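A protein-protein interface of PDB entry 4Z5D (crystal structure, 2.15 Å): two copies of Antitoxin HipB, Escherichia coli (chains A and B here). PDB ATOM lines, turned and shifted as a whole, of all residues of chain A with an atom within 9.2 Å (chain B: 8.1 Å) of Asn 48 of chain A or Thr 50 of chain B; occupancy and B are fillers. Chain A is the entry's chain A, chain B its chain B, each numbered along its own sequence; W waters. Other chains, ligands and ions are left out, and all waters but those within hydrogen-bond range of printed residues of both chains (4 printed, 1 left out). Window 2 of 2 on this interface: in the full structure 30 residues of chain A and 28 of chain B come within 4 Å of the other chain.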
ATOM      1  N   PRO A   7      24.175  18.772 -13.305  1.00  0.00           N
ATOM      2  CA  PRO A   7      22.828  18.449 -13.766  1.00  0.00           C
ATOM      3  C   PRO A   7      22.726  17.019 -14.302  1.00  0.00           C
ATOM      4  O   PRO A   7      21.766  16.354 -14.025  1.00  0.00           O
ATOM      5  CB  PRO A   7      22.572  19.476 -14.861  1.00  0.00           C
ATOM      6  CG  PRO A   7      23.419  20.613 -14.469  1.00  0.00           C
ATOM      7  CD  PRO A   7      24.659  20.014 -13.908  1.00  0.00           C
ATOM      8  N   THR A   8      23.740  16.585 -15.042  1.00  0.00           N
ATOM      9  CA  THR A   8      23.779  15.259 -15.641  1.00  0.00           C
ATOM     10  C   THR A   8      23.777  14.196 -14.571  1.00  0.00           C
ATOM     11  O   THR A   8      23.020  13.254 -14.620  1.00  0.00           O
ATOM     12  CB  THR A   8      25.051  15.075 -16.509  1.00  0.00           C
ATOM     13  OG1 THR A   8      24.994  15.930 -17.640  1.00  0.00           O
ATOM     14  CG2 THR A   8      25.204  13.637 -16.978  1.00  0.00           C
ATOM     15  N   LEU A  10      22.743  14.597 -11.531  1.00  0.00           N
ATOM     16  CA  LEU A  10      21.447  14.641 -10.884  1.00  0.00           C
ATOM     17  C   LEU A  10      20.370  13.911 -11.687  1.00  0.00           C
ATOM     18  O   LEU A  10      19.603  13.158 -11.150  1.00  0.00           O
ATOM     19  CB  LEU A  10      21.026  16.091 -10.633  1.00  0.00           C
ATOM     20  CG  LEU A  10      19.611  16.359 -10.134  1.00  0.00           C
ATOM     21  CD1 LEU A  10      19.361  15.747  -8.777  1.00  0.00           C
ATOM     22  CD2 LEU A  10      19.287  17.840 -10.141  1.00  0.00           C
ATOM     23  N   ASN A  41      13.189  15.367 -21.616  1.00  0.00           N
ATOM     24  CA  ASN A  41      14.225  16.371 -21.783  1.00  0.00           C
ATOM     25  C   ASN A  41      15.100  16.473 -20.540  1.00  0.00           C
ATOM     26  O   ASN A  41      16.291  16.612 -20.676  1.00  0.00           O
ATOM     27  CB  ASN A  41      13.676  17.735 -22.180  1.00  0.00           C
ATOM     28  CG  ASN A  41      14.776  18.755 -22.478  1.00  0.00           C
ATOM     29  OD1 ASN A  41      15.437  18.693 -23.505  1.00  0.00           O
ATOM     30  ND2 ASN A  41      14.966  19.698 -21.575  1.00  0.00           N
ATOM     31  N   PHE A  42      14.501  16.398 -19.348  1.00  0.00           N
ATOM     32  CA  PHE A  42      15.278  16.461 -18.110  1.00  0.00           C
ATOM     33  C   PHE A  42      16.251  15.296 -17.987  1.00  0.00           C
ATOM     34  O   PHE A  42      17.405  15.496 -17.721  1.00  0.00           O
ATOM     35  CB  PHE A  42      14.390  16.499 -16.851  1.00  0.00           C
ATOM     36  CG  PHE A  42      15.141  16.287 -15.551  1.00  0.00           C
ATOM     37  CD1 PHE A  42      16.006  17.243 -15.063  1.00  0.00           C
ATOM     38  CD2 PHE A  42      14.967  15.140 -14.826  1.00  0.00           C
ATOM     39  CE1 PHE A  42      16.687  17.042 -13.882  1.00  0.00           C
ATOM     40  CE2 PHE A  42      15.634  14.938 -13.643  1.00  0.00           C
ATOM     41  CZ  PHE A  42      16.498  15.889 -13.168  1.00  0.00           C
ATOM     42  N   ASN A  44      17.562  13.392 -20.238  1.00  0.00           N
ATOM     43  CA  ASN A  44      18.585  13.421 -21.262  1.00  0.00           C
ATOM     44  C   ASN A  44      19.389  14.711 -21.388  1.00  0.00           C
ATOM     45  O   ASN A  44      20.557  14.670 -21.660  1.00  0.00           O
ATOM     46  CB  ASN A  44      17.982  13.028 -22.609  1.00  0.00           C
ATOM     47  CG  ASN A  44      17.444  11.625 -22.606  1.00  0.00           C
ATOM     48  OD1 ASN A  44      18.198  10.688 -22.480  1.00  0.00           O
ATOM     49  ND2 ASN A  44      16.145  11.478 -22.710  1.00  0.00           N
ATOM     50  N   ASN A  45      18.728  15.843 -21.209  1.00  0.00           N
ATOM     51  CA  ASN A  45      19.353  17.136 -21.337  1.00  0.00           C
ATOM     52  C   ASN A  45      19.053  18.096 -20.184  1.00  0.00           C
ATOM     53  O   ASN A  45      18.418  19.091 -20.364  1.00  0.00           O
ATOM     54  CB  ASN A  45      18.947  17.751 -22.650  1.00  0.00           C
ATOM     55  CG  ASN A  45      20.117  18.304 -23.399  1.00  0.00           C
ATOM     56  OD1 ASN A  45      20.757  17.587 -24.165  1.00  0.00           O
ATOM     57  ND2 ASN A  45      20.430  19.569 -23.168  1.00  0.00           N
ATOM     58  N   PRO A  46      19.511  17.782 -18.993  1.00  0.00           N
ATOM     59  CA  PRO A  46      19.118  18.515 -17.795  1.00  0.00           C
ATOM     60  C   PRO A  46      19.681  19.942 -17.615  1.00  0.00           C
ATOM     61  O   PRO A  46      19.192  20.637 -16.745  1.00  0.00           O
ATOM     62  CB  PRO A  46      19.608  17.620 -16.680  1.00  0.00           C
ATOM     63  CG  PRO A  46      20.815  16.979 -17.243  1.00  0.00           C
ATOM     64  CD  PRO A  46      20.542  16.780 -18.701  1.00  0.00           C
ATOM     65  N   ASP A  47      20.651  20.357 -18.420  1.00  0.00           N
ATOM     66  CA  ASP A  47      21.418  21.551 -18.128  1.00  0.00           C
ATOM     67  C   ASP A  47      20.608  22.834 -18.012  1.00  0.00           C
ATOM     68  O   ASP A  47      20.833  23.594 -17.110  1.00  0.00           O
ATOM     69  CB  ASP A  47      22.487  21.778 -19.185  1.00  0.00           C
ATOM     70  CG  ASP A  47      23.726  20.997 -18.925  1.00  0.00           C
ATOM     71  OD1 ASP A  47      23.815  20.312 -17.926  1.00  0.00           O
ATOM     72  OD2 ASP A  47      24.617  21.063 -19.752  1.00  0.00           O
ATOM     73  N   ASN A  48      19.672  23.048 -18.918  1.00  0.00           N
ATOM     74  CA  ASN A  48      18.841  24.227 -18.909  1.00  0.00           C
ATOM     75  C   ASN A  48      17.454  24.011 -18.292  1.00  0.00           C
ATOM     76  O   ASN A  48      16.627  24.882 -18.330  1.00  0.00           O
ATOM     77  CB  ASN A  48      18.774  24.866 -20.290  1.00  0.00           C
ATOM     78  CG  ASN A  48      20.140  25.171 -20.861  1.00  0.00           C
ATOM     79  OD1 ASN A  48      20.817  26.076 -20.427  1.00  0.00           O
ATOM     80  ND2 ASN A  48      20.552  24.386 -21.821  1.00  0.00           N
ATOM     81  N   THR A  49      17.239  22.840 -17.719  1.00  0.00           N
ATOM     82  CA  THR A  49      16.006  22.491 -17.047  1.00  0.00           C
ATOM     83  C   THR A  49      15.766  23.452 -15.848  1.00  0.00           C
ATOM     84  O   THR A  49      16.675  23.796 -15.130  1.00  0.00           O
ATOM     85  CB  THR A  49      16.063  21.024 -16.566  1.00  0.00           C
ATOM     86  OG1 THR A  49      15.985  20.125 -17.680  1.00  0.00           O
ATOM     87  CG2 THR A  49      14.961  20.721 -15.617  1.00  0.00           C
ATOM     88  N   THR A  50      14.538  23.895 -15.675  1.00  0.00           N
ATOM     89  CA  THR A  50      14.190  24.791 -14.581  1.00  0.00           C
ATOM     90  C   THR A  50      14.203  24.130 -13.203  1.00  0.00           C
ATOM     91  O   THR A  50      13.972  22.960 -13.068  1.00  0.00           O
ATOM     92  CB  THR A  50      12.832  25.494 -14.771  1.00  0.00           C
ATOM     93  OG1 THR A  50      11.796  24.537 -14.835  1.00  0.00           O
ATOM     94  CG2 THR A  50      12.809  26.317 -16.013  1.00  0.00           C
ATOM     95  N   LEU A  51      14.415  24.941 -12.185  1.00  0.00           N
ATOM     96  CA  LEU A  51      14.356  24.493 -10.820  1.00  0.00           C
ATOM     97  C   LEU A  51      12.950  23.975 -10.493  1.00  0.00           C
ATOM     98  O   LEU A  51      12.818  23.019  -9.782  1.00  0.00           O
ATOM     99  CB  LEU A  51      14.805  25.577  -9.842  1.00  0.00           C
ATOM    100  CG  LEU A  51      16.315  25.844  -9.772  1.00  0.00           C
ATOM    101  CD1 LEU A  51      16.679  26.817  -8.680  1.00  0.00           C
ATOM    102  CD2 LEU A  51      17.137  24.578  -9.675  1.00  0.00           C
ATOM    103  N   THR A  52      11.928  24.618 -11.042  1.00  0.00           N
ATOM    104  CA  THR A  52      10.547  24.225 -10.826  1.00  0.00           C
ATOM    105  C   THR A  52      10.292  22.788 -11.335  1.00  0.00           C
ATOM    106  O   THR A  52       9.745  21.971 -10.643  1.00  0.00           O
ATOM    107  CB  THR A  52       9.551  25.187 -11.536  1.00  0.00           C
ATOM    108  OG1 THR A  52       9.589  26.475 -10.929  1.00  0.00           O
ATOM    109  CG2 THR A  52       8.149  24.669 -11.439  1.00  0.00           C
ATOM    110  N   THR A  53      10.782  22.491 -12.526  1.00  0.00           N
ATOM    111  CA  THR A  53      10.675  21.160 -13.085  1.00  0.00           C
ATOM    112  C   THR A  53      11.416  20.171 -12.214  1.00  0.00           C
ATOM    113  O   THR A  53      10.904  19.129 -11.945  1.00  0.00           O
ATOM    114  CB  THR A  53      11.245  21.066 -14.525  1.00  0.00           C
ATOM    115  OG1 THR A  53      10.405  21.764 -15.422  1.00  0.00           O
ATOM    116  CG2 THR A  53      11.333  19.641 -15.009  1.00  0.00           C
ATOM    117  N   PHE A  54      12.618  20.508 -11.784  1.00  0.00           N
ATOM    118  CA  PHE A  54      13.406  19.578 -11.012  1.00  0.00           C
ATOM    119  C   PHE A  54      12.649  19.213  -9.723  1.00  0.00           C
ATOM    120  O   PHE A  54      12.480  18.060  -9.419  1.00  0.00           O
ATOM    121  CB  PHE A  54      14.764  20.207 -10.708  1.00  0.00           C
ATOM    122  CG  PHE A  54      15.452  19.676  -9.484  1.00  0.00           C
ATOM    123  CD1 PHE A  54      15.702  18.335  -9.331  1.00  0.00           C
ATOM    124  CD2 PHE A  54      15.867  20.533  -8.501  1.00  0.00           C
ATOM    125  CE1 PHE A  54      16.348  17.857  -8.219  1.00  0.00           C
ATOM    126  CE2 PHE A  54      16.516  20.067  -7.379  1.00  0.00           C
ATOM    127  CZ  PHE A  54      16.745  18.727  -7.232  1.00  0.00           C
ATOM    128  N   THR B  38      22.762  37.345 -12.409  1.00  0.00           N
ATOM    129  CA  THR B  38      22.244  35.982 -12.434  1.00  0.00           C
ATOM    130  C   THR B  38      22.069  35.461 -11.012  1.00  0.00           C
ATOM    131  O   THR B  38      21.102  34.762 -10.707  1.00  0.00           O
ATOM    132  CB  THR B  38      23.152  35.050 -13.283  1.00  0.00           C
ATOM    133  OG1 THR B  38      23.234  35.563 -14.621  1.00  0.00           O
ATOM    134  CG2 THR B  38      22.592  33.623 -13.338  1.00  0.00           C
ATOM    135  N   ASN B  41      18.967  37.162  -9.687  1.00  0.00           N
ATOM    136  CA  ASN B  41      17.742  36.512 -10.159  1.00  0.00           C
ATOM    137  C   ASN B  41      17.476  35.202  -9.420  1.00  0.00           C
ATOM    138  O   ASN B  41      16.366  34.945  -9.079  1.00  0.00           O
ATOM    139  CB  ASN B  41      17.695  36.299 -11.675  1.00  0.00           C
ATOM    140  CG  ASN B  41      16.324  35.803 -12.160  1.00  0.00           C
ATOM    141  OD1 ASN B  41      15.382  36.567 -12.248  1.00  0.00           O
ATOM    142  ND2 ASN B  41      16.224  34.517 -12.470  1.00  0.00           N
ATOM    143  N   PHE B  42      18.507  34.404  -9.181  1.00  0.00           N
ATOM    144  CA  PHE B  42      18.345  33.139  -8.500  1.00  0.00           C
ATOM    145  C   PHE B  42      17.833  33.333  -7.064  1.00  0.00           C
ATOM    146  O   PHE B  42      16.960  32.628  -6.630  1.00  0.00           O
ATOM    147  CB  PHE B  42      19.656  32.333  -8.474  1.00  0.00           C
ATOM    148  CG  PHE B  42      19.660  31.191  -7.486  1.00  0.00           C
ATOM    149  CD1 PHE B  42      18.953  30.028  -7.736  1.00  0.00           C
ATOM    150  CD2 PHE B  42      20.326  31.298  -6.301  1.00  0.00           C
ATOM    151  CE1 PHE B  42      18.947  28.995  -6.816  1.00  0.00           C
ATOM    152  CE2 PHE B  42      20.329  30.271  -5.383  1.00  0.00           C
ATOM    153  CZ  PHE B  42      19.639  29.121  -5.638  1.00  0.00           C
ATOM    154  N   ASN B  45      14.111  35.209  -7.702  1.00  0.00           N
ATOM    155  CA  ASN B  45      13.178  34.511  -8.561  1.00  0.00           C
ATOM    156  C   ASN B  45      13.742  33.167  -9.038  1.00  0.00           C
ATOM    157  O   ASN B  45      14.009  32.961 -10.201  1.00  0.00           O
ATOM    158  CB  ASN B  45      12.806  35.397  -9.739  1.00  0.00           C
ATOM    159  CG  ASN B  45      12.403  36.795  -9.319  1.00  0.00           C
ATOM    160  OD1 ASN B  45      13.141  37.755  -9.520  1.00  0.00           O
ATOM    161  ND2 ASN B  45      11.221  36.918  -8.764  1.00  0.00           N
ATOM    162  N   PRO B  46      13.948  32.242  -8.117  1.00  0.00           N
ATOM    163  CA  PRO B  46      14.622  30.988  -8.433  1.00  0.00           C
ATOM    164  C   PRO B  46      13.829  30.004  -9.315  1.00  0.00           C
ATOM    165  O   PRO B  46      14.451  29.105  -9.804  1.00  0.00           O
ATOM    166  CB  PRO B  46      14.867  30.379  -7.069  1.00  0.00           C
ATOM    167  CG  PRO B  46      13.773  30.885  -6.244  1.00  0.00           C
ATOM    168  CD  PRO B  46      13.472  32.259  -6.727  1.00  0.00           C
ATOM    169  N   ASP B  47      12.527  30.179  -9.505  1.00  0.00           N
ATOM    170  CA  ASP B  47      11.689  29.152 -10.116  1.00  0.00           C
ATOM    171  C   ASP B  47      12.140  28.736 -11.532  1.00  0.00           C
ATOM    172  O   ASP B  47      12.218  27.570 -11.809  1.00  0.00           O
ATOM    173  CB  ASP B  47      10.226  29.614 -10.211  1.00  0.00           C
ATOM    174  CG  ASP B  47       9.466  29.510  -8.895  1.00  0.00           C
ATOM    175  OD1 ASP B  47       9.896  28.846  -7.975  1.00  0.00           O
ATOM    176  OD2 ASP B  47       8.405  30.105  -8.796  1.00  0.00           O
ATOM    177  N   ASN B  48      12.456  29.694 -12.387  1.00  0.00           N
ATOM    178  CA  ASN B  48      12.919  29.408 -13.740  1.00  0.00           C
ATOM    179  C   ASN B  48      14.449  29.310 -13.917  1.00  0.00           C
ATOM    180  O   ASN B  48      14.930  29.118 -15.006  1.00  0.00           O
ATOM    181  CB  ASN B  48      12.313  30.369 -14.769  1.00  0.00           C
ATOM    182  CG  ASN B  48      10.796  30.402 -14.742  1.00  0.00           C
ATOM    183  OD1 ASN B  48      10.129  29.446 -15.094  1.00  0.00           O
ATOM    184  ND2 ASN B  48      10.255  31.520 -14.345  1.00  0.00           N
ATOM    185  N   THR B  49      15.185  29.402 -12.819  1.00  0.00           N
ATOM    186  CA  THR B  49      16.633  29.299 -12.849  1.00  0.00           C
ATOM    187  C   THR B  49      17.052  27.923 -13.445  1.00  0.00           C
ATOM    188  O   THR B  49      16.487  26.903 -13.131  1.00  0.00           O
ATOM    189  CB  THR B  49      17.238  29.493 -11.432  1.00  0.00           C
ATOM    190  OG1 THR B  49      16.915  30.789 -10.931  1.00  0.00           O
ATOM    191  CG2 THR B  49      18.727  29.361 -11.457  1.00  0.00           C
ATOM    192  N   THR B  50      18.021  27.936 -14.329  1.00  0.00           N
ATOM    193  CA  THR B  50      18.553  26.693 -14.848  1.00  0.00           C
ATOM    194  C   THR B  50      19.296  25.877 -13.779  1.00  0.00           C
ATOM    195  O   THR B  50      19.895  26.414 -12.857  1.00  0.00           O
ATOM    196  CB  THR B  50      19.478  26.860 -16.074  1.00  0.00           C
ATOM    197  OG1 THR B  50      20.715  27.426 -15.673  1.00  0.00           O
ATOM    198  CG2 THR B  50      18.870  27.717 -17.146  1.00  0.00           C
ATOM    199  N   LEU B  51      19.283  24.572 -13.971  1.00  0.00           N
ATOM    200  CA  LEU B  51      20.015  23.659 -13.128  1.00  0.00           C
ATOM    201  C   LEU B  51      21.519  23.994 -13.180  1.00  0.00           C
ATOM    202  O   LEU B  51      22.182  23.926 -12.189  1.00  0.00           O
ATOM    203  CB  LEU B  51      19.772  22.200 -13.522  1.00  0.00           C
ATOM    204  CG  LEU B  51      18.439  21.545 -13.159  1.00  0.00           C
ATOM    205  CD1 LEU B  51      18.344  20.097 -13.581  1.00  0.00           C
ATOM    206  CD2 LEU B  51      18.111  21.688 -11.693  1.00  0.00           C
ATOM    207  N   THR B  52      22.006  24.401 -14.338  1.00  0.00           N
ATOM    208  CA  THR B  52      23.414  24.733 -14.516  1.00  0.00           C
ATOM    209  C   THR B  52      23.801  25.903 -13.592  1.00  0.00           C
ATOM    210  O   THR B  52      24.803  25.837 -12.914  1.00  0.00           O
ATOM    211  CB  THR B  52      23.755  25.068 -15.999  1.00  0.00           C
ATOM    212  OG1 THR B  52      23.774  23.875 -16.772  1.00  0.00           O
ATOM    213  CG2 THR B  52      25.099  25.701 -16.126  1.00  0.00           C
ATOM    214  N   THR B  53      22.957  26.923 -13.548  1.00  0.00           N
ATOM    215  CA  THR B  53      23.188  28.046 -12.665  1.00  0.00           C
ATOM    216  C   THR B  53      23.195  27.588 -11.192  1.00  0.00           C
ATOM    217  O   THR B  53      24.029  28.017 -10.447  1.00  0.00           O
ATOM    218  CB  THR B  53      22.181  29.197 -12.869  1.00  0.00           C
ATOM    219  OG1 THR B  53      22.412  29.842 -14.109  1.00  0.00           O
ATOM    220  CG2 THR B  53      22.301  30.233 -11.769  1.00  0.00           C
ATOM    221  N   PHE B  54      22.267  26.715 -10.817  1.00  0.00           N
ATOM    222  CA  PHE B  54      22.163  26.251  -9.449  1.00  0.00           C
ATOM    223  C   PHE B  54      23.445  25.524  -9.030  1.00  0.00           C
ATOM    224  O   PHE B  54      23.967  25.775  -7.967  1.00  0.00           O
ATOM    225  CB  PHE B  54      20.941  25.335  -9.317  1.00  0.00           C
ATOM    226  CG  PHE B  54      20.975  24.411  -8.145  1.00  0.00           C
ATOM    227  CD1 PHE B  54      21.086  24.894  -6.865  1.00  0.00           C
ATOM    228  CD2 PHE B  54      20.893  23.058  -8.333  1.00  0.00           C
ATOM    229  CE1 PHE B  54      21.118  24.042  -5.798  1.00  0.00           C
ATOM    230  CE2 PHE B  54      20.915  22.193  -7.269  1.00  0.00           C
ATOM    231  CZ  PHE B  54      21.029  22.688  -5.996  1.00  0.00           C
ATOM    232  N   PHE B  55      23.915  24.630  -9.883  1.00  0.00           N
ATOM    233  CA  PHE B  55      25.143  23.913  -9.604  1.00  0.00           C
ATOM    234  C   PHE B  55      26.402  24.784  -9.554  1.00  0.00           C
ATOM    235  O   PHE B  55      27.247  24.571  -8.729  1.00  0.00           O
ATOM    236  CB  PHE B  55      25.302  22.650 -10.450  1.00  0.00           C
ATOM    237  CG  PHE B  55      24.501  21.486  -9.949  1.00  0.00           C
ATOM    238  CD1 PHE B  55      24.912  20.757  -8.858  1.00  0.00           C
ATOM    239  CD2 PHE B  55      23.334  21.129 -10.574  1.00  0.00           C
ATOM    240  CE1 PHE B  55      24.166  19.698  -8.407  1.00  0.00           C
ATOM    241  CE2 PHE B  55      22.589  20.069 -10.128  1.00  0.00           C
ATOM    242  CZ  PHE B  55      22.994  19.359  -9.044  1.00  0.00           C
ATOM    243  N   LYS B  56      26.497  25.770 -10.423  1.00  0.00           N
ATOM    244  CA  LYS B  56      27.611  26.694 -10.374  1.00  0.00           C
ATOM    245  C   LYS B  56      27.622  27.482  -9.048  1.00  0.00           C
ATOM    246  O   LYS B  56      28.645  27.592  -8.419  1.00  0.00           O
ATOM    247  CB  LYS B  56      27.589  27.650 -11.563  1.00  0.00           C
ATOM    248  CG  LYS B  56      27.979  27.035 -12.888  1.00  0.00           C
ATOM    249  CD  LYS B  56      28.276  28.090 -13.920  1.00  0.00           C
ATOM    250  CE  LYS B  56      28.438  27.486 -15.299  1.00  0.00           C
ATOM    251  NZ  LYS B  56      28.407  28.514 -16.347  1.00  0.00           N
ATOM    252  N   ILE B  57      26.461  27.985  -8.637  1.00  0.00           N
ATOM    253  CA  ILE B  57      26.301  28.681  -7.363  1.00  0.00           C
ATOM    254  C   ILE B  57      26.574  27.793  -6.138  1.00  0.00           C
ATOM    255  O   ILE B  57      27.194  28.214  -5.194  1.00  0.00           O
ATOM    256  CB  ILE B  57      24.939  29.404  -7.225  1.00  0.00           C
ATOM    257  CG1 ILE B  57      24.734  30.404  -8.368  1.00  0.00           C
ATOM    258  CG2 ILE B  57      24.834  30.096  -5.879  1.00  0.00           C
ATOM    259  CD1 ILE B  57      23.482  31.225  -8.265  1.00  0.00           C
HETATM  260  O   HOH W   1      15.769  27.453 -17.152  1.00  0.00           O
HETATM  261  O   HOH W   2      23.582  25.729 -19.662  1.00  0.00           O
HETATM  262  O   HOH W   3       8.166  27.977 -13.308  1.00  0.00           O
HETATM  263  O   HOH W   4       8.172  26.383  -8.275  1.00  0.00           O
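O of Asp 47 of chain A is in hydrogen-bond range of OG1 of Thr 52 of chain B, at 3.0 Å. O of Thr 49 of chain A is in hydrogen-bond range of N of Leu 51 of chain B, at 3.0 Å. O of Asp 47 of chain B sits at hydrogen-bond distance from N of Leu 51 of chain A, at 3.4 Å. N of Leu 51 of chain A sits at hydrogen-bond distance from O of Thr 49 of chain B. The side-chain hydroxyl (OG1) of Thr 52 of chain A sits at hydrogen-bond distance from the backbone carbonyl oxygen (O) of Asp 47 of chain B, 3.0 Å away.
The side-chain hydroxyl (OG1) of Thr 49 of chain A lies close to the backbone carbonyl oxygen (O) of Pro 46 of chain A (3.4 Å). The side-chain hydroxyl (OG1) of Thr 50 of chain A lies within hydrogen-bond range of the side-chain hydroxyl (OG1) of Thr 53 of chain A (3.2 Å). O of Pro 46 of chain B lies within hydrogen-bond range of OG1 of Thr 49 of chain B (3.2 Å). The side-chain hydroxyl (OG1) of Thr 50 of chain B is in hydrogen-bond range of the backbone NH (N) of Thr 53 of chain B (3.1 Å).
Among the printed residues, pairs that only touch across the chains: Pro 46 of chain A with Leu 51 of chain B, Leu 51 of chain A with Pro 46 of chain B, Thr 50 of chain A with Thr 49 of chain B, Thr 49 of chain A with Thr 50 of chain B, Phe 42 of chain A with Leu 51 of chain B, Asp 47 of chain A with Leu 51 of chain B, Thr 50 of chain A with Asn 48 of chain B, Leu 51 of chain A with Phe 42 of chain B, Leu 51 of chain A with Leu 51 of chain B, Thr 50 of chain A with Asp 47 of chain B, Asp 47 of chain A with Thr 50 of chain B, Thr 49 of chain A with Thr 49 of chain B, Pro 7 of chain A with Phe 55 of chain B, Phe 54 of chain A with Leu 51 of chain B, Asn 48 of chain A with Thr 50 of chain B, Leu 51 of chain A with Phe 54 of chain B and Leu 10 of chain A with Phe 55 of chain B.
Thr 8 of chain A touches none of the printed residues of chain B. Asn 41 of chain A touches none of the printed residues of chain B. Of the printed residues of chain B, Asp 47 of chain A touches Thr 50 (3.7 Å), Leu 51 (3.6 Å) and Thr 52 (3.0 Å). Of the printed residues of chain B, Asn 48 of chain A touches Thr 50. Of the printed residues of chain B, Thr 52 of chain A touches Asp 47. Printed residues of chain B within 4 Å of Phe 54 of chain A: Leu 51. Printed residues of chain A within 4 Å of Asp 47 of chain B: Thr 50 (3.7 Å), Leu 51 (3.4 Å) and Thr 52 (3.0 Å). Thr 49 of chain B touches just these residues of chain A: Thr 49 (3.7 Å), Thr 50 (3.4 Å) and Leu 51 (3.0 Å). No residue of chain A comes within 4 Å of Thr 53 of chain B. Printed residues of chain A within 4 Å of Phe 54 of chain B: Leu 51. The nearest residue of chain A that does not touch Thr 50 of chain B is Leu 51 of chain A (4.6 Å). The nearest printed residue of chain A that does not touch Asn 48 of chain B is Thr 52 of chain A (4.6 Å).
Of the 16 printed residues of chain A, 11 touch a printed residue of chain B. Hydrophobic or aromatic side chains of chain A that line the printed part of chain B: Pro 7, Leu 10, Phe 42, Leu 51 and Phe 54. Printed residues of chain B that touch a printed residue of chain A: Phe 42, Pro 46, Asp 47, Asn 48, Thr 49, Thr 50, Leu 51, Thr 52, Phe 54 and Phe 55. Hydrophobic or aromatic side chains of chain B within 4 Å of the printed part of chain A: Phe 42, Leu 51, Phe 54 and Phe 55.
Pro 46 of chain A touches Leu 51 of chain B, and with the chains exchanged Leu 51 of chain A touches Pro 46 of chain B. Asp 47 of chain A touches Leu 51 of chain B, and with the chains exchanged Leu 51 of chain A touches Asp 47 of chain B. Thr 49 of chain A touches Thr 50 of chain B, and with the chains exchanged Thr 50 of chain A touches Thr 49 of chain B. Leu 51 of chain A touches Phe 54 of chain B, and with the chains exchanged Phe 54 of chain A touches Leu 51 of chain B. 12 positions are printed for both chains.
Water W1 lies within hydrogen-bond range of the backbone carbonyl oxygen of Asn 48 of chain B (2.8 Å) and the backbone carbonyl oxygen of Asn 48 of chain A (3.0 Å). Water W2 lies within hydrogen-bond range of OD1 of Asn 48 of chain A (2.9 Å) and OG1 of Thr 52 of chain B (3.4 Å). Water W4 bridges OG1 of Thr 52 of chain A (3.0 Å) and OD1 of Asp 47 of chain B (3.0 Å). Water W3 bridges the side-chain amide oxygen (OD1) of Asn 48 of chain B (3.0 Å) and the side-chain hydroxyl (OG1) of Thr 52 of chain A (3.2 Å).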
